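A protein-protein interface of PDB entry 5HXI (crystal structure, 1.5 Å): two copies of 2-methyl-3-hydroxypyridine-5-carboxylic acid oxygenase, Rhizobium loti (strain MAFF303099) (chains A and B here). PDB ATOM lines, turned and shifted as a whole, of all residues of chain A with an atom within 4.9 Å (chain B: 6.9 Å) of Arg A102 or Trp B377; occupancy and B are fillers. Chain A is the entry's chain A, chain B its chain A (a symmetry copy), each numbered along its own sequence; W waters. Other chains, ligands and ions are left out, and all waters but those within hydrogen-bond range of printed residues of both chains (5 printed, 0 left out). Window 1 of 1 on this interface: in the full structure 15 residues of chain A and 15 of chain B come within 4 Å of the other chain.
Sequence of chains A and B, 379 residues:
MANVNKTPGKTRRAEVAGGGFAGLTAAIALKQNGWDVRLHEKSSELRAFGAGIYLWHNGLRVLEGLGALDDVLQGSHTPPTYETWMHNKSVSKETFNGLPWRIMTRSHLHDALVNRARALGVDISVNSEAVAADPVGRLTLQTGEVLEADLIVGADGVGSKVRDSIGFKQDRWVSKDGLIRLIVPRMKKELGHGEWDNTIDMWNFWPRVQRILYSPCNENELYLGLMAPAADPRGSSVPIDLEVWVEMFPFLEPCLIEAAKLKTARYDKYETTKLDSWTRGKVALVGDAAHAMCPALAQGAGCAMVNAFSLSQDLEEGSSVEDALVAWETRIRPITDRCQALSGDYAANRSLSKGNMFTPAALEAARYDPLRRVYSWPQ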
ATOM      1  N   ILE A  53     -25.472  -4.917  32.785  1.00  0.00           N
ATOM      2  CA  ILE A  53     -25.780  -6.101  33.572  1.00  0.00           C
ATOM      3  C   ILE A  53     -24.636  -7.111  33.524  1.00  0.00           C
ATOM      4  O   ILE A  53     -23.972  -7.260  32.499  1.00  0.00           O
ATOM      5  CB  ILE A  53     -27.116  -6.747  33.111  1.00  0.00           C
ATOM      6  CG1 ILE A  53     -27.611  -7.776  34.133  1.00  0.00           C
ATOM      7  CG2 ILE A  53     -27.000  -7.358  31.718  1.00  0.00           C
ATOM      8  CD1 ILE A  53     -29.024  -8.248  33.875  1.00  0.00           C
ATOM      9  N   TYR A  54     -24.414  -7.771  34.659  1.00  0.00           N
ATOM     10  CA  TYR A  54     -23.467  -8.879  34.782  1.00  0.00           C
ATOM     11  C   TYR A  54     -24.226 -10.199  34.687  1.00  0.00           C
ATOM     12  O   TYR A  54     -25.275 -10.350  35.313  1.00  0.00           O
ATOM     13  CB  TYR A  54     -22.774  -8.860  36.150  1.00  0.00           C
ATOM     14  CG  TYR A  54     -21.724  -7.788  36.367  1.00  0.00           C
ATOM     15  CD1 TYR A  54     -22.021  -6.430  36.225  1.00  0.00           C
ATOM     16  CD2 TYR A  54     -20.435  -8.134  36.772  1.00  0.00           C
ATOM     17  CE1 TYR A  54     -21.054  -5.457  36.440  1.00  0.00           C
ATOM     18  CE2 TYR A  54     -19.466  -7.166  36.995  1.00  0.00           C
ATOM     19  CZ  TYR A  54     -19.778  -5.830  36.825  1.00  0.00           C
ATOM     20  OH  TYR A  54     -18.809  -4.877  37.048  1.00  0.00           O
ATOM     21  N   LEU A  55     -23.692 -11.148  33.924  1.00  0.00           N
ATOM     22  CA  LEU A  55     -24.124 -12.542  34.005  1.00  0.00           C
ATOM     23  C   LEU A  55     -22.935 -13.404  34.390  1.00  0.00           C
ATOM     24  O   LEU A  55     -21.774 -13.039  34.159  1.00  0.00           O
ATOM     25  CB  LEU A  55     -24.719 -13.030  32.684  1.00  0.00           C
ATOM     26  CG  LEU A  55     -26.044 -12.406  32.231  1.00  0.00           C
ATOM     27  CD1 LEU A  55     -26.472 -13.038  30.915  1.00  0.00           C
ATOM     28  CD2 LEU A  55     -27.146 -12.549  33.273  1.00  0.00           C
ATOM     29  N   LEU A  60     -25.184 -17.729  31.813  1.00  0.00           N
ATOM     30  CA  LEU A  60     -24.598 -18.062  30.513  1.00  0.00           C
ATOM     31  C   LEU A  60     -25.001 -19.470  30.068  1.00  0.00           C
ATOM     32  O   LEU A  60     -25.226 -19.706  28.878  1.00  0.00           O
ATOM     33  CB  LEU A  60     -23.073 -17.917  30.542  1.00  0.00           C
ATOM     34  CG  LEU A  60     -22.544 -16.497  30.789  1.00  0.00           C
ATOM     35  CD1 LEU A  60     -21.053 -16.522  31.094  1.00  0.00           C
ATOM     36  CD2 LEU A  60     -22.832 -15.576  29.612  1.00  0.00           C
ATOM     37  N   LEU A  73     -22.472 -13.393  23.665  1.00  0.00           N
ATOM     38  CA  LEU A  73     -21.006 -13.315  23.787  1.00  0.00           C
ATOM     39  C   LEU A  73     -20.376 -12.364  22.765  1.00  0.00           C
ATOM     40  O   LEU A  73     -19.439 -11.631  23.089  1.00  0.00           O
ATOM     41  CB  LEU A  73     -20.360 -14.705  23.701  1.00  0.00           C
ATOM     42  CG  LEU A  73     -20.648 -15.683  24.846  1.00  0.00           C
ATOM     43  CD1 LEU A  73     -19.870 -16.971  24.631  1.00  0.00           C
ATOM     44  CD2 LEU A  73     -20.324 -15.093  26.213  1.00  0.00           C
ATOM     45  N   GLN A  74     -20.896 -12.374  21.541  1.00  0.00           N
ATOM     46  CA  GLN A  74     -20.503 -11.394  20.534  1.00  0.00           C
ATOM     47  C   GLN A  74     -20.952 -10.011  20.992  1.00  0.00           C
ATOM     48  O   GLN A  74     -22.138  -9.798  21.211  1.00  0.00           O
ATOM     49  CB  GLN A  74     -21.137 -11.733  19.179  1.00  0.00           C
ATOM     50  CG  GLN A  74     -20.722 -10.828  18.024  1.00  0.00           C
ATOM     51  CD  GLN A  74     -19.238 -10.918  17.703  1.00  0.00           C
ATOM     52  OE1 GLN A  74     -18.684 -12.012  17.594  1.00  0.00           O
ATOM     53  NE2 GLN A  74     -18.589  -9.768  17.546  1.00  0.00           N
ATOM     54  N   SER A  76     -20.012  -8.465  23.895  1.00  0.00           N
ATOM     55  CA  SER A  76     -19.966  -8.325  25.354  1.00  0.00           C
ATOM     56  C   SER A  76     -18.541  -8.634  25.842  1.00  0.00           C
ATOM     57  O   SER A  76     -17.679  -8.995  25.039  1.00  0.00           O
ATOM     58  CB  SER A  76     -21.020  -9.215  26.017  1.00  0.00           C
ATOM     59  OG  SER A  76     -20.778 -10.579  25.766  1.00  0.00           O
ATOM     60  N   HIS A  77     -18.299  -8.499  27.146  1.00  0.00           N
ATOM     61  CA  HIS A  77     -16.940  -8.387  27.691  1.00  0.00           C
ATOM     62  C   HIS A  77     -16.774  -9.229  28.949  1.00  0.00           C
ATOM     63  O   HIS A  77     -17.624  -9.181  29.828  1.00  0.00           O
ATOM     64  CB  HIS A  77     -16.709  -6.904  28.016  1.00  0.00           C
ATOM     65  CG  HIS A  77     -15.372  -6.579  28.607  1.00  0.00           C
ATOM     66  ND1 HIS A  77     -14.216  -6.543  27.860  1.00  0.00           N
ATOM     67  CD2 HIS A  77     -15.021  -6.203  29.859  1.00  0.00           C
ATOM     68  CE1 HIS A  77     -13.206  -6.184  28.631  1.00  0.00           C
ATOM     69  NE2 HIS A  77     -13.667  -5.970  29.850  1.00  0.00           N
ATOM     70  N   THR A  78     -15.693 -10.013  29.024  1.00  0.00           N
ATOM     71  CA  THR A  78     -15.251 -10.583  30.301  1.00  0.00           C
ATOM     72  C   THR A  78     -14.009  -9.809  30.719  1.00  0.00           C
ATOM     73  O   THR A  78     -12.981  -9.904  30.051  1.00  0.00           O
ATOM     74  CB  THR A  78     -14.895 -12.087  30.224  1.00  0.00           C
ATOM     75  OG1 THR A  78     -16.022 -12.837  29.753  1.00  0.00           O
ATOM     76  CG2 THR A  78     -14.493 -12.609  31.605  1.00  0.00           C
ATOM     77  N   PRO A 100     -16.948 -18.837  34.481  1.00  0.00           N
ATOM     78  CA  PRO A 100     -17.315 -17.852  33.456  1.00  0.00           C
ATOM     79  C   PRO A 100     -18.190 -16.703  33.946  1.00  0.00           C
ATOM     80  O   PRO A 100     -19.071 -16.902  34.783  1.00  0.00           O
ATOM     81  CB  PRO A 100     -18.076 -18.686  32.424  1.00  0.00           C
ATOM     82  CG  PRO A 100     -17.484 -20.042  32.546  1.00  0.00           C
ATOM     83  CD  PRO A 100     -17.175 -20.215  34.003  1.00  0.00           C
ATOM     84  N   TRP A 101     -17.921 -15.509  33.430  1.00  0.00           N
ATOM     85  CA  TRP A 101     -18.758 -14.345  33.690  1.00  0.00           C
ATOM     86  C   TRP A 101     -18.651 -13.359  32.542  1.00  0.00           C
ATOM     87  O   TRP A 101     -17.783 -13.486  31.673  1.00  0.00           O
ATOM     88  CB  TRP A 101     -18.414 -13.696  35.035  1.00  0.00           C
ATOM     89  CG  TRP A 101     -17.018 -13.169  35.176  1.00  0.00           C
ATOM     90  CD1 TRP A 101     -15.857 -13.885  35.130  1.00  0.00           C
ATOM     91  CD2 TRP A 101     -16.641 -11.813  35.445  1.00  0.00           C
ATOM     92  NE1 TRP A 101     -14.779 -13.058  35.327  1.00  0.00           N
ATOM     93  CE2 TRP A 101     -15.231 -11.780  35.525  1.00  0.00           C
ATOM     94  CE3 TRP A 101     -17.359 -10.618  35.615  1.00  0.00           C
ATOM     95  CZ2 TRP A 101     -14.523 -10.601  35.777  1.00  0.00           C
ATOM     96  CZ3 TRP A 101     -16.653  -9.446  35.861  1.00  0.00           C
ATOM     97  CH2 TRP A 101     -15.249  -9.449  35.946  1.00  0.00           C
ATOM     98  N   ARG A 102     -19.561 -12.393  32.528  1.00  0.00           N
ATOM     99  CA  ARG A 102     -19.716 -11.511  31.380  1.00  0.00           C
ATOM    100  C   ARG A 102     -20.432 -10.234  31.770  1.00  0.00           C
ATOM    101  O   ARG A 102     -21.331 -10.263  32.607  1.00  0.00           O
ATOM    102  CB  ARG A 102     -20.524 -12.225  30.287  1.00  0.00           C
ATOM    103  CG  ARG A 102     -20.256 -11.719  28.880  1.00  0.00           C
ATOM    104  CD  ARG A 102     -18.878 -12.143  28.416  1.00  0.00           C
ATOM    105  NE  ARG A 102     -18.680 -11.980  26.983  1.00  0.00           N
ATOM    106  CZ  ARG A 102     -17.583 -12.369  26.332  1.00  0.00           C
ATOM    107  NH1 ARG A 102     -16.567 -12.928  26.989  1.00  0.00           N
ATOM    108  NH2 ARG A 102     -17.502 -12.203  25.018  1.00  0.00           N
ATOM    109  N   ILE A 103     -20.036  -9.128  31.146  1.00  0.00           N
ATOM    110  CA  ILE A 103     -20.714  -7.843  31.301  1.00  0.00           C
ATOM    111  C   ILE A 103     -21.233  -7.425  29.935  1.00  0.00           C
ATOM    112  O   ILE A 103     -20.579  -7.640  28.915  1.00  0.00           O
ATOM    113  CB  ILE A 103     -19.772  -6.750  31.851  1.00  0.00           C
ATOM    114  CG1 ILE A 103     -19.115  -7.211  33.154  1.00  0.00           C
ATOM    115  CG2 ILE A 103     -20.529  -5.440  32.070  1.00  0.00           C
ATOM    116  CD1 ILE A 103     -18.075  -6.256  33.684  1.00  0.00           C
ATOM    117  N   MET A 104     -22.409  -6.813  29.924  1.00  0.00           N
ATOM    118  CA  MET A 104     -23.035  -6.369  28.682  1.00  0.00           C
ATOM    119  C   MET A 104     -24.033  -5.269  28.992  1.00  0.00           C
ATOM    120  O   MET A 104     -24.445  -5.107  30.144  1.00  0.00           O
ATOM    121  CB  MET A 104     -23.753  -7.540  28.018  1.00  0.00           C
ATOM    122  CG  MET A 104     -24.909  -8.099  28.838  1.00  0.00           C
ATOM    123  SD  MET A 104     -25.239  -9.838  28.534  1.00  0.00           S
ATOM    124  CE  MET A 104     -23.825 -10.587  29.339  1.00  0.00           C
ATOM    125  N   HIS B  57     -11.125 -24.171  26.160  1.00  0.00           N
ATOM    126  CA  HIS B  57     -12.552 -24.339  25.883  1.00  0.00           C
ATOM    127  C   HIS B  57     -12.877 -25.580  25.037  1.00  0.00           C
ATOM    128  O   HIS B  57     -13.731 -26.378  25.419  1.00  0.00           O
ATOM    129  CB  HIS B  57     -13.078 -23.048  25.236  1.00  0.00           C
ATOM    130  CG  HIS B  57     -14.379 -23.196  24.516  1.00  0.00           C
ATOM    131  ND1 HIS B  57     -14.455 -23.285  23.144  1.00  0.00           N
ATOM    132  CD2 HIS B  57     -15.654 -23.252  24.969  1.00  0.00           C
ATOM    133  CE1 HIS B  57     -15.719 -23.397  22.782  1.00  0.00           C
ATOM    134  NE2 HIS B  57     -16.468 -23.376  23.869  1.00  0.00           N
ATOM    135  N   ARG B  61     -14.892 -28.620  26.593  1.00  0.00           N
ATOM    136  CA  ARG B  61     -16.170 -29.027  26.004  1.00  0.00           C
ATOM    137  C   ARG B  61     -16.195 -30.516  25.649  1.00  0.00           C
ATOM    138  O   ARG B  61     -17.213 -31.175  25.853  1.00  0.00           O
ATOM    139  CB  ARG B  61     -16.517 -28.165  24.784  1.00  0.00           C
ATOM    140  CG  ARG B  61     -16.878 -26.725  25.131  1.00  0.00           C
ATOM    141  CD  ARG B  61     -18.222 -26.597  25.831  1.00  0.00           C
ATOM    142  NE  ARG B  61     -19.344 -26.684  24.902  1.00  0.00           N
ATOM    143  CZ  ARG B  61     -20.622 -26.526  25.247  1.00  0.00           C
ATOM    144  NH1 ARG B  61     -20.966 -26.320  26.518  1.00  0.00           N
ATOM    145  NH2 ARG B  61     -21.566 -26.593  24.312  1.00  0.00           N
ATOM    146  N   PHE B  96      -7.860 -13.653  27.143  1.00  0.00           N
ATOM    147  CA  PHE B  96      -8.600 -14.291  26.045  1.00  0.00           C
ATOM    148  C   PHE B  96     -10.104 -13.971  26.030  1.00  0.00           C
ATOM    149  O   PHE B  96     -10.911 -14.794  25.593  1.00  0.00           O
ATOM    150  CB  PHE B  96      -8.383 -15.819  26.080  1.00  0.00           C
ATOM    151  CG  PHE B  96      -6.984 -16.234  26.466  1.00  0.00           C
ATOM    152  CD1 PHE B  96      -5.892 -15.853  25.698  1.00  0.00           C
ATOM    153  CD2 PHE B  96      -6.760 -17.001  27.607  1.00  0.00           C
ATOM    154  CE1 PHE B  96      -4.606 -16.229  26.059  1.00  0.00           C
ATOM    155  CE2 PHE B  96      -5.475 -17.381  27.967  1.00  0.00           C
ATOM    156  CZ  PHE B  96      -4.398 -16.997  27.191  1.00  0.00           C
ATOM    157  N   ASN B  97     -10.468 -12.778  26.507  1.00  0.00           N
ATOM    158  CA  ASN B  97     -11.862 -12.354  26.546  1.00  0.00           C
ATOM    159  C   ASN B  97     -12.795 -13.431  27.133  1.00  0.00           C
ATOM    160  O   ASN B  97     -13.846 -13.744  26.557  1.00  0.00           O
ATOM    161  CB  ASN B  97     -12.296 -11.940  25.132  1.00  0.00           C
ATOM    162  CG  ASN B  97     -11.412 -10.846  24.554  1.00  0.00           C
ATOM    163  OD1 ASN B  97     -10.521 -11.104  23.737  1.00  0.00           O
ATOM    164  ND2 ASN B  97     -11.637  -9.620  24.999  1.00  0.00           N
ATOM    165  N   GLY B  98     -12.387 -14.016  28.257  1.00  0.00           N
ATOM    166  CA  GLY B  98     -13.201 -14.997  28.963  1.00  0.00           C
ATOM    167  C   GLY B  98     -13.198 -16.422  28.440  1.00  0.00           C
ATOM    168  O   GLY B  98     -13.849 -17.273  29.035  1.00  0.00           O
ATOM    169  N   LEU B  99     -12.483 -16.690  27.344  1.00  0.00           N
ATOM    170  CA  LEU B  99     -12.365 -18.045  26.793  1.00  0.00           C
ATOM    171  C   LEU B  99     -11.898 -18.996  27.897  1.00  0.00           C
ATOM    172  O   LEU B  99     -10.830 -18.783  28.465  1.00  0.00           O
ATOM    173  CB  LEU B  99     -11.354 -18.060  25.643  1.00  0.00           C
ATOM    174  CG  LEU B  99     -11.006 -19.382  24.952  1.00  0.00           C
ATOM    175  CD1 LEU B  99     -12.149 -19.849  24.069  1.00  0.00           C
ATOM    176  CD2 LEU B  99      -9.736 -19.214  24.135  1.00  0.00           C
ATOM    177  N   PRO B 100     -12.694 -20.046  28.214  1.00  0.00           N
ATOM    178  CA  PRO B 100     -12.241 -20.948  29.281  1.00  0.00           C
ATOM    179  C   PRO B 100     -10.920 -21.662  29.009  1.00  0.00           C
ATOM    180  O   PRO B 100     -10.646 -22.056  27.875  1.00  0.00           O
ATOM    181  CB  PRO B 100     -13.376 -21.968  29.384  1.00  0.00           C
ATOM    182  CG  PRO B 100     -14.582 -21.213  28.961  1.00  0.00           C
ATOM    183  CD  PRO B 100     -14.113 -20.280  27.885  1.00  0.00           C
ATOM    184  N   LEU B 363      -6.083 -18.585  18.540  1.00  0.00           N
ATOM    185  CA  LEU B 363      -7.114 -19.203  19.381  1.00  0.00           C
ATOM    186  C   LEU B 363      -8.235 -19.928  18.617  1.00  0.00           C
ATOM    187  O   LEU B 363      -9.190 -20.375  19.248  1.00  0.00           O
ATOM    188  CB  LEU B 363      -7.736 -18.143  20.304  1.00  0.00           C
ATOM    189  CG  LEU B 363      -6.808 -17.537  21.360  1.00  0.00           C
ATOM    190  CD1 LEU B 363      -7.464 -16.325  22.005  1.00  0.00           C
ATOM    191  CD2 LEU B 363      -6.432 -18.563  22.421  1.00  0.00           C
ATOM    192  N   ALA B 366      -8.962 -23.403  19.984  1.00  0.00           N
ATOM    193  CA  ALA B 366      -9.514 -23.242  21.332  1.00  0.00           C
ATOM    194  C   ALA B 366     -10.968 -22.772  21.325  1.00  0.00           C
ATOM    195  O   ALA B 366     -11.766 -23.209  22.156  1.00  0.00           O
ATOM    196  CB  ALA B 366      -8.661 -22.279  22.139  1.00  0.00           C
ATOM    197  N   ARG B 367     -11.299 -21.894  20.378  1.00  0.00           N
ATOM    198  CA  ARG B 367     -12.647 -21.337  20.263  1.00  0.00           C
ATOM    199  C   ARG B 367     -13.696 -22.320  19.746  1.00  0.00           C
ATOM    200  O   ARG B 367     -14.893 -22.104  19.952  1.00  0.00           O
ATOM    201  CB  ARG B 367     -12.634 -20.099  19.362  1.00  0.00           C
ATOM    202  CG  ARG B 367     -11.924 -18.904  19.981  1.00  0.00           C
ATOM    203  CD  ARG B 367     -11.923 -17.708  19.053  1.00  0.00           C
ATOM    204  NE  ARG B 367     -13.307 -17.316  18.806  1.00  0.00           N
ATOM    205  CZ  ARG B 367     -13.958 -17.368  17.641  1.00  0.00           C
ATOM    206  NH1 ARG B 367     -13.364 -17.751  16.508  1.00  0.00           N
ATOM    207  NH2 ARG B 367     -15.238 -17.006  17.607  1.00  0.00           N
ATOM    208  N   TYR B 375     -17.964 -22.006  16.489  1.00  0.00           N
ATOM    209  CA  TYR B 375     -16.935 -21.271  17.222  1.00  0.00           C
ATOM    210  C   TYR B 375     -17.605 -20.344  18.225  1.00  0.00           C
ATOM    211  O   TYR B 375     -18.574 -19.660  17.889  1.00  0.00           O
ATOM    212  CB  TYR B 375     -16.041 -20.485  16.268  1.00  0.00           C
ATOM    213  CG  TYR B 375     -15.235 -21.375  15.359  1.00  0.00           C
ATOM    214  CD1 TYR B 375     -13.991 -21.858  15.754  1.00  0.00           C
ATOM    215  CD2 TYR B 375     -15.717 -21.747  14.107  1.00  0.00           C
ATOM    216  CE1 TYR B 375     -13.245 -22.684  14.924  1.00  0.00           C
ATOM    217  CE2 TYR B 375     -14.977 -22.570  13.267  1.00  0.00           C
ATOM    218  CZ  TYR B 375     -13.744 -23.036  13.682  1.00  0.00           C
ATOM    219  OH  TYR B 375     -13.012 -23.848  12.845  1.00  0.00           O
ATOM    220  N   SER B 376     -17.094 -20.340  19.454  1.00  0.00           N
ATOM    221  CA  SER B 376     -17.641 -19.532  20.544  1.00  0.00           C
ATOM    222  C   SER B 376     -16.565 -18.572  21.047  1.00  0.00           C
ATOM    223  O   SER B 376     -15.513 -18.432  20.418  1.00  0.00           O
ATOM    224  CB  SER B 376     -18.139 -20.449  21.667  1.00  0.00           C
ATOM    225  OG  SER B 376     -18.847 -19.728  22.662  1.00  0.00           O
ATOM    226  N   TRP B 377     -16.849 -17.887  22.154  1.00  0.00           N
ATOM    227  CA  TRP B 377     -15.891 -16.999  22.827  1.00  0.00           C
ATOM    228  C   TRP B 377     -15.121 -16.099  21.853  1.00  0.00           C
ATOM    229  O   TRP B 377     -13.896 -16.214  21.720  1.00  0.00           O
ATOM    230  CB  TRP B 377     -14.962 -17.820  23.728  1.00  0.00           C
ATOM    231  CG  TRP B 377     -15.751 -18.514  24.782  1.00  0.00           C
ATOM    232  CD1 TRP B 377     -16.149 -19.820  24.785  1.00  0.00           C
ATOM    233  CD2 TRP B 377     -16.310 -17.921  25.957  1.00  0.00           C
ATOM    234  NE1 TRP B 377     -16.899 -20.083  25.903  1.00  0.00           N
ATOM    235  CE2 TRP B 377     -17.020 -18.934  26.639  1.00  0.00           C
ATOM    236  CE3 TRP B 377     -16.274 -16.631  26.508  1.00  0.00           C
ATOM    237  CZ2 TRP B 377     -17.681 -18.700  27.851  1.00  0.00           C
ATOM    238  CZ3 TRP B 377     -16.933 -16.398  27.710  1.00  0.00           C
ATOM    239  CH2 TRP B 377     -17.629 -17.430  28.366  1.00  0.00           C
ATOM    240  N   PRO B 378     -15.849 -15.211  21.146  1.00  0.00           N
ATOM    241  CA  PRO B 378     -15.230 -14.343  20.141  1.00  0.00           C
ATOM    242  C   PRO B 378     -14.226 -13.361  20.743  1.00  0.00           C
ATOM    243  O   PRO B 378     -14.367 -12.961  21.896  1.00  0.00           O
ATOM    244  CB  PRO B 378     -16.425 -13.604  19.528  1.00  0.00           C
ATOM    245  CG  PRO B 378     -17.465 -13.623  20.592  1.00  0.00           C
ATOM    246  CD  PRO B 378     -17.296 -14.945  21.273  1.00  0.00           C
ATOM    247  N   GLN B 379     -13.232 -12.978  19.948  1.00  0.00           N
ATOM    248  CA  GLN B 379     -12.107 -12.170  20.416  1.00  0.00           C
ATOM    249  C   GLN B 379     -12.150 -10.745  19.862  1.00  0.00           C
ATOM    250  O   GLN B 379     -13.173 -10.279  19.366  1.00  0.00           O
ATOM    251  CB  GLN B 379     -10.800 -12.855  20.013  1.00  0.00           C
ATOM    252  CG  GLN B 379     -10.641 -14.266  20.555  1.00  0.00           C
ATOM    253  CD  GLN B 379     -10.502 -14.297  22.067  1.00  0.00           C
ATOM    254  OE1 GLN B 379      -9.607 -13.667  22.622  1.00  0.00           O
ATOM    255  NE2 GLN B 379     -11.388 -15.028  22.741  1.00  0.00           N
ATOM    256  OXT GLN B 379     -11.155 -10.016  19.901  1.00  0.00           O
HETATM  257  O   HOH W   1     -11.039 -12.017  30.021  1.00  0.00           O
HETATM  258  O   HOH W   2     -13.798  -9.409  26.734  1.00  0.00           O
HETATM  259  O   HOH W   3     -15.338 -14.077  24.208  1.00  0.00           O
HETATM  260  O   HOH W   4     -15.875 -10.097  18.263  1.00  0.00           O
HETATM  261  O   HOH W   5     -15.569 -15.919  31.210  1.00  0.00           O
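Among the printed residues, merely in contact across the chains: Gln A74 with Pro B378 (3.4 Å), Leu A73 with Ser B376 (3.5 Å), Arg A102 with Trp B377 (3.6 Å), Thr A78 with Gly B98 (3.6 Å), Leu A73 with Pro B378 (3.8 Å), Leu A73 with Trp B377 (3.9 Å) and Thr A78 with Asn B97 (3.97 Å).
The guanidinium group of Arg A102 sits at hydrogen-bond distance from the backbone carbonyl oxygen of Asn B97, at 2.9 Å.
1 position is printed for both chains.
Of the 8 pairs that touch across the chains among the printed residues, none has its exchanged pair printed and touching as well.
Of the printed residues of chain B, Leu A73 touches Ser B376, Trp B377 and Pro B378.
Of the printed residues of chain B, Gln A74 touches Pro B378 (3.4 Å).
Of the printed residues of chain B, Thr A78 touches Asn B97 (3.97 Å) and Gly B98 (3.6 Å).
Of the printed residues of chain B, Arg A102 touches Asn B97 and Trp B377.
Ile A103 touches none of the printed residues of chain B.
Arg B61 touches none of the printed residues of chain A.
Of the printed residues of chain A, Asn B97 touches Thr A78 (3.97 Å) and Arg A102 (2.9 Å).
Of chain A, only Leu A73 (3.9 Å) and Arg A102 (3.6 Å) come within 4 Å of Trp B377.
Of the printed residues of chain A, Pro B378 touches Leu A73 and Gln A74.
The nearest printed residue of chain B that does not touch Arg A102 is Gly B98 (4.4 Å).
The nearest residue of chain A that does not touch Trp B377 is Thr A78 (4.2 Å).
The nearest printed residue of chain A that does not touch Asn B97 is His A77 (4.9 Å).
Of the 15 printed residues of chain B, 5 touch a printed residue of chain A.
Printed residues of chain B that touch a printed residue of chain A: Asn B97, Gly B98, Ser B376, Trp B377 and Pro B378.
Hydrophobic or aromatic side chains of chain B that line the printed part of chain A: Trp B377 and Pro B378.
Hydrophobic or aromatic side chains of chain A that line the printed part of chain B: Leu A73.
Along chain A the printed residues that touch a printed residue of chain B span positions 73 to 102.
Among the printed residues, 8 pairs touch across the chains.
Water W3 lies within hydrogen-bond range of the backbone carbonyl oxygen (O) of Pro B378 (2.7 Å), the backbone carbonyl oxygen (O) of Asn B97 (2.8 Å) and the guanidinium group (NH2) of Arg A102 (3.0 Å).
Water W2 lies within hydrogen-bond range of the side-chain amide nitrogen (ND2) of Asn B97 (2.8 Å), the backbone NH (N) of Thr A78 (3.0 Å) and a ring nitrogen (ND1) of His A77 (3.1 Å).
Water W4 bridges NE2 of Gln A74 (2.8 Å) and O of Gln B379 (2.9 Å).
Water W1 lies within hydrogen-bond range of the backbone carbonyl oxygen of Thr A78 (2.9 Å) and the backbone NH of Gly B98 (3.0 Å).
Water W5 lies within hydrogen-bond range of O of Gly B98, N of Trp A101 and OG1 of Thr A78.
O of Leu A55 sits at hydrogen-bond distance from N of Arg A102, at 2.8 Å.
The side-chain hydroxyl (OG) of Ser A76 is in hydrogen-bond range of the guanidinium group (NE) of Arg A102 (2.8 Å).
The side-chain hydroxyl (OG1) of Thr A78 sits at hydrogen-bond distance from the backbone carbonyl oxygen (O) of Trp A101 (2.7 Å).
The backbone carbonyl oxygen (O) of Arg B367 sits at hydrogen-bond distance from the backbone NH (N) of Ser B376.
NE of Arg B367 lies within hydrogen-bond range of O of Trp B377, 3.2 Å away.
NE2 of Gln B379 lies within hydrogen-bond range of O of Trp B377, at 3.0 Å.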
